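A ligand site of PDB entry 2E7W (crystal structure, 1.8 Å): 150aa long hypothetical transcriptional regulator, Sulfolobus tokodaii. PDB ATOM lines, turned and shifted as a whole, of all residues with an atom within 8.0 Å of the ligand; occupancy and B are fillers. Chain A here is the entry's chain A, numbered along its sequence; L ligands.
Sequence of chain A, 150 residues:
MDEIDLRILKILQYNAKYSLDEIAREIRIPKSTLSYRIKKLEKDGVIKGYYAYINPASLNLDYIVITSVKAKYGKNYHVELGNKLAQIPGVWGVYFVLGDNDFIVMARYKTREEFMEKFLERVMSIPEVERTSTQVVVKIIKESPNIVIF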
ATOM      1  N   LEU A  20     -10.555  27.832  21.777  1.00  0.00           N
ATOM      2  CA  LEU A  20     -10.472  27.199  20.471  1.00  0.00           C
ATOM      3  C   LEU A  20     -10.489  25.679  20.620  1.00  0.00           C
ATOM      4  O   LEU A  20     -11.083  24.972  19.816  1.00  0.00           O
ATOM      5  CB  LEU A  20      -9.192  27.622  19.743  1.00  0.00           C
ATOM      6  CG  LEU A  20      -9.152  29.019  19.121  1.00  0.00           C
ATOM      7  CD1 LEU A  20     -10.150  29.092  17.971  1.00  0.00           C
ATOM      8  CD2 LEU A  20      -9.450  30.073  20.171  1.00  0.00           C
ATOM      9  N   ASP A  21      -9.829  25.176  21.668  1.00  0.00           N
ATOM     10  CA  ASP A  21      -9.764  23.744  21.920  1.00  0.00           C
ATOM     11  C   ASP A  21     -11.158  23.147  22.078  1.00  0.00           C
ATOM     12  O   ASP A  21     -11.487  22.134  21.456  1.00  0.00           O
ATOM     13  CB  ASP A  21      -8.942  23.466  23.187  1.00  0.00           C
ATOM     14  CG  ASP A  21      -7.481  23.828  23.024  1.00  0.00           C
ATOM     15  OD1 ASP A  21      -7.183  24.977  22.654  1.00  0.00           O
ATOM     16  OD2 ASP A  21      -6.622  22.950  23.284  1.00  0.00           O
ATOM     17  N   GLU A  22     -11.972  23.790  22.910  1.00  0.00           N
ATOM     18  CA  GLU A  22     -13.330  23.322  23.169  1.00  0.00           C
ATOM     19  C   GLU A  22     -14.187  23.297  21.898  1.00  0.00           C
ATOM     20  O   GLU A  22     -14.802  22.275  21.581  1.00  0.00           O
ATOM     21  CB  GLU A  22     -13.990  24.225  24.216  1.00  0.00           C
ATOM     22  CG  GLU A  22     -13.223  24.280  25.531  1.00  0.00           C
ATOM     23  CD  GLU A  22     -13.871  25.182  26.556  1.00  0.00           C
ATOM     24  OE1 GLU A  22     -13.917  26.413  26.336  1.00  0.00           O
ATOM     25  OE2 GLU A  22     -14.342  24.666  27.597  1.00  0.00           O
ATOM     26  N   ILE A  23     -14.234  24.410  21.187  1.00  0.00           N
ATOM     27  CA  ILE A  23     -15.015  24.490  19.960  1.00  0.00           C
ATOM     28  C   ILE A  23     -14.509  23.489  18.929  1.00  0.00           C
ATOM     29  O   ILE A  23     -15.301  22.819  18.263  1.00  0.00           O
ATOM     30  CB  ILE A  23     -14.972  25.905  19.362  1.00  0.00           C
ATOM     31  CG1 ILE A  23     -15.480  26.916  20.383  1.00  0.00           C
ATOM     32  CG2 ILE A  23     -15.824  25.956  18.088  1.00  0.00           C
ATOM     33  CD1 ILE A  23     -15.401  28.357  19.921  1.00  0.00           C
ATOM     34  N   ALA A  24     -13.187  23.389  18.800  1.00  0.00           N
ATOM     35  CA  ALA A  24     -12.594  22.475  17.843  1.00  0.00           C
ATOM     36  C   ALA A  24     -13.064  21.048  18.138  1.00  0.00           C
ATOM     37  O   ALA A  24     -13.344  20.284  17.218  1.00  0.00           O
ATOM     38  CB  ALA A  24     -11.073  22.545  17.917  1.00  0.00           C
ATOM     39  N   ARG A  25     -13.155  20.715  19.420  1.00  0.00           N
ATOM     40  CA  ARG A  25     -13.594  19.386  19.819  1.00  0.00           C
ATOM     41  C   ARG A  25     -15.091  19.203  19.522  1.00  0.00           C
ATOM     42  O   ARG A  25     -15.504  18.152  19.064  1.00  0.00           O
ATOM     43  CB  ARG A  25     -13.370  19.166  21.316  1.00  0.00           C
ATOM     44  CG  ARG A  25     -12.443  18.005  21.633  1.00  0.00           C
ATOM     45  CD  ARG A  25     -12.680  17.470  23.049  1.00  0.00           C
ATOM     46  NE  ARG A  25     -12.669  18.542  24.040  1.00  0.00           N
ATOM     47  CZ  ARG A  25     -11.606  19.275  24.336  1.00  0.00           C
ATOM     48  NH1 ARG A  25     -10.452  19.062  23.718  1.00  0.00           N
ATOM     49  NH2 ARG A  25     -11.688  20.237  25.246  1.00  0.00           N
ATOM     50  N   ARG A  28     -15.434  19.186  15.522  1.00  0.00           N
ATOM     51  CA  ARG A  28     -14.597  18.203  14.829  1.00  0.00           C
ATOM     52  C   ARG A  28     -13.701  18.725  13.704  1.00  0.00           C
ATOM     53  O   ARG A  28     -13.693  18.167  12.607  1.00  0.00           O
ATOM     54  CB  ARG A  28     -15.467  17.071  14.278  1.00  0.00           C
ATOM     55  CG  ARG A  28     -15.904  16.040  15.309  1.00  0.00           C
ATOM     56  CD  ARG A  28     -16.480  16.695  16.551  1.00  0.00           C
ATOM     57  NE  ARG A  28     -16.973  15.723  17.513  1.00  0.00           N
ATOM     58  CZ  ARG A  28     -16.247  14.716  18.011  1.00  0.00           C
ATOM     59  NH1 ARG A  28     -14.987  14.541  17.626  1.00  0.00           N
ATOM     60  NH2 ARG A  28     -16.780  13.879  18.879  1.00  0.00           N
ATOM     61  N   ILE A  29     -12.963  19.802  13.965  1.00  0.00           N
ATOM     62  CA  ILE A  29     -12.050  20.333  12.965  1.00  0.00           C
ATOM     63  C   ILE A  29     -10.778  20.783  13.664  1.00  0.00           C
ATOM     64  O   ILE A  29     -10.777  21.033  14.874  1.00  0.00           O
ATOM     65  CB  ILE A  29     -12.648  21.537  12.185  1.00  0.00           C
ATOM     66  CG1 ILE A  29     -12.921  22.706  13.131  1.00  0.00           C
ATOM     67  CG2 ILE A  29     -13.932  21.114  11.483  1.00  0.00           C
ATOM     68  CD1 ILE A  29     -13.309  23.976  12.417  1.00  0.00           C
ATOM     69  N   PRO A  30      -9.663  20.875  12.917  1.00  0.00           N
ATOM     70  CA  PRO A  30      -8.405  21.304  13.526  1.00  0.00           C
ATOM     71  C   PRO A  30      -8.524  22.705  14.119  1.00  0.00           C
ATOM     72  O   PRO A  30      -9.160  23.579  13.538  1.00  0.00           O
ATOM     73  CB  PRO A  30      -7.414  21.250  12.355  1.00  0.00           C
ATOM     74  CG  PRO A  30      -7.976  20.153  11.507  1.00  0.00           C
ATOM     75  CD  PRO A  30      -9.451  20.445  11.529  1.00  0.00           C
ATOM     76  N   LYS A  31      -7.933  22.894  15.293  1.00  0.00           N
ATOM     77  CA  LYS A  31      -7.950  24.171  15.995  1.00  0.00           C
ATOM     78  C   LYS A  31      -7.446  25.304  15.092  1.00  0.00           C
ATOM     79  O   LYS A  31      -7.977  26.415  15.126  1.00  0.00           O
ATOM     80  CB  LYS A  31      -7.074  24.093  17.251  1.00  0.00           C
ATOM     81  CG  LYS A  31      -6.996  25.373  18.056  1.00  0.00           C
ATOM     82  CD  LYS A  31      -6.047  25.208  19.241  1.00  0.00           C
ATOM     83  CE  LYS A  31      -5.968  26.483  20.071  1.00  0.00           C
ATOM     84  NZ  LYS A  31      -5.026  26.345  21.224  1.00  0.00           N
ATOM     85  N   SER A  32      -6.431  25.014  14.288  1.00  0.00           N
ATOM     86  CA  SER A  32      -5.864  26.007  13.384  1.00  0.00           C
ATOM     87  C   SER A  32      -6.858  26.339  12.273  1.00  0.00           C
ATOM     88  O   SER A  32      -6.916  27.462  11.797  1.00  0.00           O
ATOM     89  CB  SER A  32      -4.553  25.481  12.778  1.00  0.00           C
ATOM     90  OG  SER A  32      -4.724  24.227  12.145  1.00  0.00           O
ATOM     91  N   THR A  33      -7.652  25.344  11.868  1.00  0.00           N
ATOM     92  CA  THR A  33      -8.662  25.548  10.830  1.00  0.00           C
ATOM     93  C   THR A  33      -9.760  26.425  11.405  1.00  0.00           C
ATOM     94  O   THR A  33     -10.302  27.297  10.727  1.00  0.00           O
ATOM     95  CB  THR A  33      -9.274  24.207  10.367  1.00  0.00           C
ATOM     96  OG1 THR A  33      -8.250  23.395   9.787  1.00  0.00           O
ATOM     97  CG2 THR A  33     -10.360  24.458   9.338  1.00  0.00           C
ATOM     98  N   LEU A  34     -10.098  26.184  12.676  1.00  0.00           N
ATOM     99  CA  LEU A  34     -11.122  26.952  13.369  1.00  0.00           C
ATOM    100  C   LEU A  34     -10.657  28.394  13.480  1.00  0.00           C
ATOM    101  O   LEU A  34     -11.387  29.325  13.135  1.00  0.00           O
ATOM    102  CB  LEU A  34     -11.361  26.377  14.761  1.00  0.00           C
ATOM    103  CG  LEU A  34     -12.283  27.175  15.690  1.00  0.00           C
ATOM    104  CD1 LEU A  34     -13.682  27.265  15.098  1.00  0.00           C
ATOM    105  CD2 LEU A  34     -12.315  26.527  17.061  1.00  0.00           C
ATOM    106  N   SER A  35      -9.439  28.586  13.964  1.00  0.00           N
ATOM    107  CA  SER A  35      -8.873  29.931  14.123  1.00  0.00           C
ATOM    108  C   SER A  35      -8.938  30.693  12.803  1.00  0.00           C
ATOM    109  O   SER A  35      -9.229  31.887  12.782  1.00  0.00           O
ATOM    110  CB  SER A  35      -7.438  29.861  14.613  1.00  0.00           C
ATOM    111  OG  SER A  35      -6.918  31.154  14.868  1.00  0.00           O
HETATM  112  N1  LIG L   1      -2.878  20.224  14.540  1.00  0.00           N
HETATM  113  C1  LIG L   1      -4.078  20.783  15.224  1.00  0.00           C
HETATM  114  C2  LIG L   1      -4.340  22.238  14.809  1.00  0.00           C
HETATM  115  O1  LIG L   1      -3.374  22.926  14.425  1.00  0.00           O
HETATM  116  C3  LIG L   1      -3.875  20.702  16.741  1.00  0.00           C
HETATM  117  C4  LIG L   1      -4.909  21.444  17.554  1.00  0.00           C
HETATM  118  C5  LIG L   1      -6.310  20.887  17.391  1.00  0.00           C
HETATM  119  O2  LIG L   1      -7.199  21.218  18.175  1.00  0.00           O
HETATM  120  N2  LIG L   1      -6.518  20.044  16.391  1.00  0.00           N
HETATM  121  O3  LIG L   1      -5.503  22.664  14.897  1.00  0.00           O
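O1 of the ligand is in hydrogen-bond range of OG of Ser 32.
The backbone NH (N) of Ser 32 sits at hydrogen-bond distance from an oxygen (O3) of the ligand.
An oxygen (O3) of the ligand is in hydrogen-bond range of the backbone NH (N) of Lys 31, at 2.5 Å.
The side-chain amino group of Lys 31 lies within salt-bridge range of the side-chain carboxylate of Asp 21, at 2.9 Å.
Pro 30 touches the ligand.
Hydrophobic or aromatic side chains that line the ligand: Pro 30.
The nearest printed residue that does not touch the ligand is Ala 24 (4.1 Å).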
